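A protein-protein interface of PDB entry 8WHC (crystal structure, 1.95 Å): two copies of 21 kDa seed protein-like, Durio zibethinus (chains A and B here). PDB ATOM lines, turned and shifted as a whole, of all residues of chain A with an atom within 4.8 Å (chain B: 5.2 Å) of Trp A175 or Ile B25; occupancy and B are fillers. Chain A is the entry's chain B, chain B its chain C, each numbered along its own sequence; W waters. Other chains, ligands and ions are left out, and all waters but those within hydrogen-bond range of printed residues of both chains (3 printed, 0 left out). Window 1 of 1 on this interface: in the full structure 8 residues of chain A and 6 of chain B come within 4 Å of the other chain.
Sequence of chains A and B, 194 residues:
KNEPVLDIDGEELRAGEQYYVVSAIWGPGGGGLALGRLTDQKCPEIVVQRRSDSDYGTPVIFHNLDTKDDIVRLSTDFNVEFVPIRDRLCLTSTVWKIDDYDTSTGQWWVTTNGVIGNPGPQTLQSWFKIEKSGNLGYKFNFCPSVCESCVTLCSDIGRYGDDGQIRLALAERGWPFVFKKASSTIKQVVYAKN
Printed residues of chain B that touch a printed residue of chain A: Ile B25, Trp B26, Gly B27, Leu B136 and Trp B175. Hydrophobic or aromatic side chains of chain B that line the printed part of chain A: Ile B25, Trp B26, Leu B136 and Trp B175. Hydrophobic or aromatic side chains of chain A that line the printed part of chain B: Ile A25, Pro A28, Trp A175 and Pro A176. Among the printed residues, no Asp or Glu carboxylate lies within 4 Å of a Lys or Arg side-chain nitrogen of the other chain.
The side-chain amide oxygen (OE1) of Gln A49 is in hydrogen-bond range of the guanidinium group (NH1) of Arg A159 (2.8 Å). OG of Ser A23 sits at hydrogen-bond distance from NE1 of Trp A175 (2.9 Å). The indole nitrogen of Trp B175 lies within hydrogen-bond range of the side-chain hydroxyl of Ser B23 (2.9 Å). The backbone carbonyl oxygen of Ile A25 sits at hydrogen-bond distance from the side-chain hydroxyl of Ser A23, at 2.6 Å. The side-chain hydroxyl of Ser B23 lies within hydrogen-bond range of the backbone carbonyl oxygen of Ile B25, at 2.7 Å. The backbone carbonyl oxygen (O) of Gly A29 lies within hydrogen-bond range of the guanidinium group (NH1) of Arg A159, 3.4 Å away.
Among the printed residues, merely in contact across the chains: Ile A25 with Trp B26, Ile A25 with Leu B136, Pro A28 with Ile B25, Pro A28 with Trp B175, Arg A159 with Ile B25, Arg A159 with Gly B27, Gly A174 with Trp B26, Trp A175 with Ile B25, Trp A175 with Trp B26 and Pro A176 with Trp B26.
Ser A23 touches none of the printed residues of chain B. Printed residues of chain B within 4 Å of Ile A25: Trp B26 (3.9 Å) and Leu B136 (3.7 Å). Printed residues of chain B within 4 Å of Trp A175: Ile B25 and Trp B26. Phe A177 touches none of the printed residues of chain B. Of chain A, only Pro A28 (3.3 Å), Arg A159 (3.7 Å) and Trp A175 (3.8 Å) come within 4 Å of Ile B25. Printed residues of chain A within 4 Å of Trp B175: Pro A28.
NH2 of Arg A159 sits at hydrogen-bond distance from O of Trp B26. The backbone carbonyl oxygen (O) of Arg A173 lies within hydrogen-bond range of the indole nitrogen (NE1) of Trp B26 (2.9 Å).
Water W2 lies within hydrogen-bond range of the guanidinium group (NH2) of Arg A173 (2.8 Å) and the backbone carbonyl oxygen (O) of Ala B24 (2.8 Å). Water W1 lies within hydrogen-bond range of O of Ser B23 and NH1 of Arg A173. Water W3 lies within hydrogen-bond range of N of Arg A159 (3.1 Å), O of Arg A173 (3.1 Å) and NE1 of Trp B26 (3.3 Å).
Trp A175 touches Ile B25, but with the chains exchanged Ile A25 does not touch Trp B175 (8.7 Å). Of the 12 pairs that touch across the chains among the printed residues, none has its exchanged pair printed and touching as well.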
ATOM      1  N   SER A  23      -9.305   9.891   0.573  1.00  0.00           N
ATOM      2  CA  SER A  23      -9.505   9.072  -0.616  1.00  0.00           C
ATOM      3  C   SER A  23      -9.115   7.635  -0.335  1.00  0.00           C
ATOM      4  O   SER A  23      -8.043   7.374   0.208  1.00  0.00           O
ATOM      5  CB  SER A  23      -8.666   9.597  -1.774  1.00  0.00           C
ATOM      6  OG  SER A  23      -8.767   8.703  -2.867  1.00  0.00           O
ATOM      7  N   ILE A  25      -8.455   5.696  -2.680  1.00  0.00           N
ATOM      8  CA  ILE A  25      -7.429   5.445  -3.683  1.00  0.00           C
ATOM      9  C   ILE A  25      -6.319   6.445  -3.410  1.00  0.00           C
ATOM     10  O   ILE A  25      -6.521   7.656  -3.555  1.00  0.00           O
ATOM     11  CB  ILE A  25      -7.970   5.597  -5.114  1.00  0.00           C
ATOM     12  CG1 ILE A  25      -9.060   4.555  -5.392  1.00  0.00           C
ATOM     13  CG2 ILE A  25      -6.840   5.465  -6.130  1.00  0.00           C
ATOM     14  CD1 ILE A  25      -9.915   4.866  -6.618  1.00  0.00           C
ATOM     15  N   PRO A  28      -1.674   8.850  -6.843  1.00  0.00           N
ATOM     16  CA  PRO A  28      -2.318   9.883  -7.661  1.00  0.00           C
ATOM     17  C   PRO A  28      -3.799  10.070  -7.324  1.00  0.00           C
ATOM     18  O   PRO A  28      -4.377  11.096  -7.695  1.00  0.00           O
ATOM     19  CB  PRO A  28      -2.097   9.378  -9.095  1.00  0.00           C
ATOM     20  CG  PRO A  28      -1.857   7.879  -8.933  1.00  0.00           C
ATOM     21  CD  PRO A  28      -1.173   7.713  -7.637  1.00  0.00           C
ATOM     22  N   GLY A  29      -4.412   9.130  -6.600  1.00  0.00           N
ATOM     23  CA  GLY A  29      -5.769   9.317  -6.108  1.00  0.00           C
ATOM     24  C   GLY A  29      -5.910  10.420  -5.079  1.00  0.00           C
ATOM     25  O   GLY A  29      -7.027  10.896  -4.851  1.00  0.00           O
ATOM     26  N   GLN A  49      -9.954  18.720  -2.274  1.00  0.00           N
ATOM     27  CA  GLN A  49      -9.202  17.548  -1.865  1.00  0.00           C
ATOM     28  C   GLN A  49      -7.715  17.856  -1.942  1.00  0.00           C
ATOM     29  O   GLN A  49      -7.241  18.383  -2.955  1.00  0.00           O
ATOM     30  CB  GLN A  49      -9.510  16.322  -2.740  1.00  0.00           C
ATOM     31  CG  GLN A  49      -8.642  15.144  -2.373  1.00  0.00           C
ATOM     32  CD  GLN A  49      -8.594  14.070  -3.444  1.00  0.00           C
ATOM     33  OE1 GLN A  49      -8.674  14.359  -4.639  1.00  0.00           O
ATOM     34  NE2 GLN A  49      -8.397  12.828  -3.019  1.00  0.00           N
ATOM     35  N   TYR A 138     -16.277   4.160   0.754  1.00  0.00           N
ATOM     36  CA  TYR A 138     -17.617   4.713   0.731  1.00  0.00           C
ATOM     37  C   TYR A 138     -17.647   5.915  -0.193  1.00  0.00           C
ATOM     38  O   TYR A 138     -16.632   6.571  -0.410  1.00  0.00           O
ATOM     39  CB  TYR A 138     -18.062   5.139   2.117  1.00  0.00           C
ATOM     40  CG  TYR A 138     -18.135   4.042   3.158  1.00  0.00           C
ATOM     41  CD1 TYR A 138     -19.264   3.240   3.273  1.00  0.00           C
ATOM     42  CD2 TYR A 138     -17.086   3.835   4.063  1.00  0.00           C
ATOM     43  CE1 TYR A 138     -19.353   2.247   4.253  1.00  0.00           C
ATOM     44  CE2 TYR A 138     -17.154   2.833   5.038  1.00  0.00           C
ATOM     45  CZ  TYR A 138     -18.301   2.048   5.127  1.00  0.00           C
ATOM     46  OH  TYR A 138     -18.391   1.067   6.100  1.00  0.00           O
ATOM     47  N   LYS A 139     -18.816   6.207  -0.744  1.00  0.00           N
ATOM     48  CA  LYS A 139     -18.969   7.396  -1.554  1.00  0.00           C
ATOM     49  C   LYS A 139     -20.095   8.248  -0.984  1.00  0.00           C
ATOM     50  O   LYS A 139     -21.057   7.727  -0.415  1.00  0.00           O
ATOM     51  CB  LYS A 139     -19.242   7.031  -3.020  1.00  0.00           C
ATOM     52  CG  LYS A 139     -20.500   6.162  -3.240  1.00  0.00           C
ATOM     53  CD  LYS A 139     -20.809   6.011  -4.735  1.00  0.00           C
ATOM     54  CE  LYS A 139     -21.964   5.015  -4.988  1.00  0.00           C
ATOM     55  NZ  LYS A 139     -22.065   4.638  -6.429  1.00  0.00           N
ATOM     56  N   PHE A 140     -19.954   9.561  -1.120  1.00  0.00           N
ATOM     57  CA  PHE A 140     -21.065  10.451  -0.838  1.00  0.00           C
ATOM     58  C   PHE A 140     -22.017  10.449  -2.021  1.00  0.00           C
ATOM     59  O   PHE A 140     -21.620  10.222  -3.173  1.00  0.00           O
ATOM     60  CB  PHE A 140     -20.585  11.872  -0.554  1.00  0.00           C
ATOM     61  CG  PHE A 140     -19.799  11.993   0.727  1.00  0.00           C
ATOM     62  CD1 PHE A 140     -18.433  11.758   0.738  1.00  0.00           C
ATOM     63  CD2 PHE A 140     -20.431  12.289   1.915  1.00  0.00           C
ATOM     64  CE1 PHE A 140     -17.708  11.851   1.912  1.00  0.00           C
ATOM     65  CE2 PHE A 140     -19.729  12.381   3.094  1.00  0.00           C
ATOM     66  CZ  PHE A 140     -18.356  12.164   3.092  1.00  0.00           C
ATOM     67  N   ILE A 157     -21.283  11.856  -5.602  1.00  0.00           N
ATOM     68  CA  ILE A 157     -20.363  12.980  -5.537  1.00  0.00           C
ATOM     69  C   ILE A 157     -18.994  12.512  -5.995  1.00  0.00           C
ATOM     70  O   ILE A 157     -18.468  11.513  -5.492  1.00  0.00           O
ATOM     71  CB  ILE A 157     -20.322  13.576  -4.129  1.00  0.00           C
ATOM     72  CG1 ILE A 157     -21.674  14.269  -3.923  1.00  0.00           C
ATOM     73  CG2 ILE A 157     -19.099  14.515  -3.998  1.00  0.00           C
ATOM     74  CD1 ILE A 157     -21.974  14.603  -2.555  1.00  0.00           C
ATOM     75  N   GLY A 158     -18.449  13.202  -6.984  1.00  0.00           N
ATOM     76  CA  GLY A 158     -17.144  12.857  -7.496  1.00  0.00           C
ATOM     77  C   GLY A 158     -16.171  14.011  -7.387  1.00  0.00           C
ATOM     78  O   GLY A 158     -16.396  14.973  -6.632  1.00  0.00           O
ATOM     79  N   ARG A 159     -15.093  13.924  -8.159  1.00  0.00           N
ATOM     80  CA  ARG A 159     -14.018  14.907  -8.157  1.00  0.00           C
ATOM     81  C   ARG A 159     -13.979  15.617  -9.505  1.00  0.00           C
ATOM     82  O   ARG A 159     -14.148  14.985 -10.551  1.00  0.00           O
ATOM     83  CB  ARG A 159     -12.668  14.234  -7.896  1.00  0.00           C
ATOM     84  CG  ARG A 159     -12.573  13.396  -6.611  1.00  0.00           C
ATOM     85  CD  ARG A 159     -11.121  12.885  -6.364  1.00  0.00           C
ATOM     86  NE  ARG A 159     -10.519  12.310  -7.560  1.00  0.00           N
ATOM     87  CZ  ARG A 159      -9.231  12.385  -7.879  1.00  0.00           C
ATOM     88  NH1 ARG A 159      -8.373  13.068  -7.142  1.00  0.00           N
ATOM     89  NH2 ARG A 159      -8.804  11.803  -8.997  1.00  0.00           N
ATOM     90  N   ARG A 173     -19.968   8.770 -11.392  1.00  0.00           N
ATOM     91  CA  ARG A 173     -19.207   7.733 -10.700  1.00  0.00           C
ATOM     92  C   ARG A 173     -18.600   8.311  -9.427  1.00  0.00           C
ATOM     93  O   ARG A 173     -17.561   8.973  -9.482  1.00  0.00           O
ATOM     94  CB  ARG A 173     -18.115   7.165 -11.602  1.00  0.00           C
ATOM     95  CG  ARG A 173     -17.353   5.996 -10.992  1.00  0.00           C
ATOM     96  CD  ARG A 173     -16.278   5.553 -11.973  1.00  0.00           C
ATOM     97  NE  ARG A 173     -15.470   4.431 -11.512  1.00  0.00           N
ATOM     98  CZ  ARG A 173     -14.488   3.900 -12.227  1.00  0.00           C
ATOM     99  NH1 ARG A 173     -14.120   4.426 -13.388  1.00  0.00           N
ATOM    100  NH2 ARG A 173     -13.837   2.842 -11.754  1.00  0.00           N
ATOM    101  N   GLY A 174     -19.207   8.012  -8.283  1.00  0.00           N
ATOM    102  CA  GLY A 174     -18.761   8.614  -7.038  1.00  0.00           C
ATOM    103  C   GLY A 174     -17.312   8.289  -6.714  1.00  0.00           C
ATOM    104  O   GLY A 174     -16.777   7.256  -7.113  1.00  0.00           O
ATOM    105  N   TRP A 175     -16.665   9.208  -5.956  1.00  0.00           N
ATOM    106  CA  TRP A 175     -15.278   8.962  -5.536  1.00  0.00           C
ATOM    107  C   TRP A 175     -15.260   8.211  -4.213  1.00  0.00           C
ATOM    108  O   TRP A 175     -16.006   8.569  -3.294  1.00  0.00           O
ATOM    109  CB  TRP A 175     -14.493  10.258  -5.388  1.00  0.00           C
ATOM    110  CG  TRP A 175     -13.025   9.962  -5.324  1.00  0.00           C
ATOM    111  CD1 TRP A 175     -12.232   9.954  -4.211  1.00  0.00           C
ATOM    112  CD2 TRP A 175     -12.201   9.536  -6.416  1.00  0.00           C
ATOM    113  NE1 TRP A 175     -10.937   9.565  -4.559  1.00  0.00           N
ATOM    114  CE2 TRP A 175     -10.902   9.312  -5.907  1.00  0.00           C
ATOM    115  CE3 TRP A 175     -12.435   9.338  -7.785  1.00  0.00           C
ATOM    116  CZ2 TRP A 175      -9.841   8.894  -6.720  1.00  0.00           C
ATOM    117  CZ3 TRP A 175     -11.370   8.934  -8.591  1.00  0.00           C
ATOM    118  CH2 TRP A 175     -10.095   8.717  -8.052  1.00  0.00           C
ATOM    119  N   PRO A 176     -14.432   7.182  -4.071  1.00  0.00           N
ATOM    120  CA  PRO A 176     -14.433   6.404  -2.829  1.00  0.00           C
ATOM    121  C   PRO A 176     -13.553   7.036  -1.759  1.00  0.00           C
ATOM    122  O   PRO A 176     -12.426   7.466  -2.020  1.00  0.00           O
ATOM    123  CB  PRO A 176     -13.874   5.052  -3.272  1.00  0.00           C
ATOM    124  CG  PRO A 176     -12.956   5.409  -4.390  1.00  0.00           C
ATOM    125  CD  PRO A 176     -13.549   6.594  -5.093  1.00  0.00           C
ATOM    126  N   PHE A 177     -14.069   7.041  -0.536  1.00  0.00           N
ATOM    127  CA  PHE A 177     -13.398   7.636   0.612  1.00  0.00           C
ATOM    128  C   PHE A 177     -13.437   6.651   1.768  1.00  0.00           C
ATOM    129  O   PHE A 177     -14.294   5.762   1.817  1.00  0.00           O
ATOM    130  CB  PHE A 177     -14.091   8.925   1.069  1.00  0.00           C
ATOM    131  CG  PHE A 177     -13.956  10.062   0.118  1.00  0.00           C
ATOM    132  CD1 PHE A 177     -12.797  10.831   0.103  1.00  0.00           C
ATOM    133  CD2 PHE A 177     -14.999  10.379  -0.753  1.00  0.00           C
ATOM    134  CE1 PHE A 177     -12.674  11.901  -0.745  1.00  0.00           C
ATOM    135  CE2 PHE A 177     -14.882  11.440  -1.626  1.00  0.00           C
ATOM    136  CZ  PHE A 177     -13.708  12.209  -1.623  1.00  0.00           C
ATOM    137  N   SER B  23      -8.090   5.519 -18.121  1.00  0.00           N
ATOM    138  CA  SER B  23      -7.428   5.729 -16.840  1.00  0.00           C
ATOM    139  C   SER B  23      -8.210   5.055 -15.720  1.00  0.00           C
ATOM    140  O   SER B  23      -9.424   5.246 -15.596  1.00  0.00           O
ATOM    141  CB  SER B  23      -7.286   7.216 -16.539  1.00  0.00           C
ATOM    142  OG  SER B  23      -6.788   7.381 -15.223  1.00  0.00           O
ATOM    143  N   ALA B  24      -7.498   4.283 -14.893  1.00  0.00           N
ATOM    144  CA  ALA B  24      -8.100   3.666 -13.717  1.00  0.00           C
ATOM    145  C   ALA B  24      -8.470   4.679 -12.650  1.00  0.00           C
ATOM    146  O   ALA B  24      -9.220   4.340 -11.726  1.00  0.00           O
ATOM    147  CB  ALA B  24      -7.146   2.630 -13.126  1.00  0.00           C
ATOM    148  N   ILE B  25      -7.948   5.896 -12.743  1.00  0.00           N
ATOM    149  CA  ILE B  25      -8.202   6.972 -11.797  1.00  0.00           C
ATOM    150  C   ILE B  25      -8.976   8.025 -12.565  1.00  0.00           C
ATOM    151  O   ILE B  25      -8.449   8.620 -13.516  1.00  0.00           O
ATOM    152  CB  ILE B  25      -6.891   7.530 -11.215  1.00  0.00           C
ATOM    153  CG1 ILE B  25      -6.235   6.442 -10.355  1.00  0.00           C
ATOM    154  CG2 ILE B  25      -7.149   8.802 -10.412  1.00  0.00           C
ATOM    155  CD1 ILE B  25      -4.820   6.729  -9.964  1.00  0.00           C
ATOM    156  N   TRP B  26     -10.242   8.220 -12.203  1.00  0.00           N
ATOM    157  CA  TRP B  26     -11.112   9.055 -13.004  1.00  0.00           C
ATOM    158  C   TRP B  26     -11.214  10.442 -12.364  1.00  0.00           C
ATOM    159  O   TRP B  26     -10.328  10.849 -11.607  1.00  0.00           O
ATOM    160  CB  TRP B  26     -12.468   8.355 -13.200  1.00  0.00           C
ATOM    161  CG  TRP B  26     -13.253   8.109 -11.958  1.00  0.00           C
ATOM    162  CD1 TRP B  26     -14.362   8.809 -11.541  1.00  0.00           C
ATOM    163  CD2 TRP B  26     -13.059   7.060 -11.002  1.00  0.00           C
ATOM    164  NE1 TRP B  26     -14.839   8.281 -10.360  1.00  0.00           N
ATOM    165  CE2 TRP B  26     -14.068   7.202 -10.014  1.00  0.00           C
ATOM    166  CE3 TRP B  26     -12.136   6.014 -10.877  1.00  0.00           C
ATOM    167  CZ2 TRP B  26     -14.158   6.348  -8.913  1.00  0.00           C
ATOM    168  CZ3 TRP B  26     -12.225   5.176  -9.784  1.00  0.00           C
ATOM    169  CH2 TRP B  26     -13.233   5.343  -8.819  1.00  0.00           C
ATOM    170  N   GLY B  27     -12.278  11.185 -12.685  1.00  0.00           N
ATOM    171  CA  GLY B  27     -12.345  12.590 -12.348  1.00  0.00           C
ATOM    172  C   GLY B  27     -11.213  13.366 -13.007  1.00  0.00           C
ATOM    173  O   GLY B  27     -11.022  13.318 -14.226  1.00  0.00           O
ATOM    174  N   GLY B  29      -8.250  12.568 -12.981  1.00  0.00           N
ATOM    175  CA  GLY B  29      -7.371  11.569 -13.572  1.00  0.00           C
ATOM    176  C   GLY B  29      -7.572  11.365 -15.058  1.00  0.00           C
ATOM    177  O   GLY B  29      -6.761  10.673 -15.680  1.00  0.00           O
ATOM    178  N   GLY B  30      -8.643  11.922 -15.632  1.00  0.00           N
ATOM    179  CA  GLY B  30      -8.835  11.921 -17.065  1.00  0.00           C
ATOM    180  C   GLY B  30      -9.485  10.662 -17.591  1.00  0.00           C
ATOM    181  O   GLY B  30      -9.945   9.780 -16.852  1.00  0.00           O
ATOM    182  N   LEU B 136      -5.396  -1.615  -8.450  1.00  0.00           N
ATOM    183  CA  LEU B 136      -6.155  -0.678  -9.271  1.00  0.00           C
ATOM    184  C   LEU B 136      -5.572  -0.676 -10.677  1.00  0.00           C
ATOM    185  O   LEU B 136      -4.733   0.159 -11.007  1.00  0.00           O
ATOM    186  CB  LEU B 136      -6.132   0.735  -8.674  1.00  0.00           C
ATOM    187  CG  LEU B 136      -7.421   1.495  -8.993  1.00  0.00           C
ATOM    188  CD1 LEU B 136      -8.547   1.001  -8.111  1.00  0.00           C
ATOM    189  CD2 LEU B 136      -7.251   2.987  -8.832  1.00  0.00           C
ATOM    190  N   TRP B 175       1.375   4.993 -14.654  1.00  0.00           N
ATOM    191  CA  TRP B 175      -0.006   5.421 -14.450  1.00  0.00           C
ATOM    192  C   TRP B 175      -0.952   4.247 -14.712  1.00  0.00           C
ATOM    193  O   TRP B 175      -0.732   3.472 -15.649  1.00  0.00           O
ATOM    194  CB  TRP B 175      -0.348   6.584 -15.378  1.00  0.00           C
ATOM    195  CG  TRP B 175      -1.719   7.177 -15.114  1.00  0.00           C
ATOM    196  CD1 TRP B 175      -2.897   6.822 -15.709  1.00  0.00           C
ATOM    197  CD2 TRP B 175      -2.033   8.209 -14.180  1.00  0.00           C
ATOM    198  NE1 TRP B 175      -3.933   7.588 -15.210  1.00  0.00           N
ATOM    199  CE2 TRP B 175      -3.426   8.440 -14.262  1.00  0.00           C
ATOM    200  CE3 TRP B 175      -1.271   8.977 -13.293  1.00  0.00           C
ATOM    201  CZ2 TRP B 175      -4.069   9.404 -13.487  1.00  0.00           C
ATOM    202  CZ3 TRP B 175      -1.913   9.935 -12.526  1.00  0.00           C
ATOM    203  CH2 TRP B 175      -3.298  10.133 -12.621  1.00  0.00           C
ATOM    204  N   PRO B 176      -1.998   4.087 -13.898  1.00  0.00           N
ATOM    205  CA  PRO B 176      -2.882   2.922 -14.030  1.00  0.00           C
ATOM    206  C   PRO B 176      -4.021   3.088 -15.033  1.00  0.00           C
ATOM    207  O   PRO B 176      -4.705   4.113 -15.098  1.00  0.00           O
ATOM    208  CB  PRO B 176      -3.427   2.759 -12.603  1.00  0.00           C
ATOM    209  CG  PRO B 176      -3.472   4.140 -12.070  1.00  0.00           C
ATOM    210  CD  PRO B 176      -2.243   4.833 -12.646  1.00  0.00           C
HETATM  211  O   HOH W   1     -11.745   3.675 -14.951  1.00  0.00           O
HETATM  212  O   HOH W   2     -11.153   2.416 -12.525  1.00  0.00           O
HETATM  213  O   HOH W   3     -15.703  11.452  -9.871  1.00  0.00           O
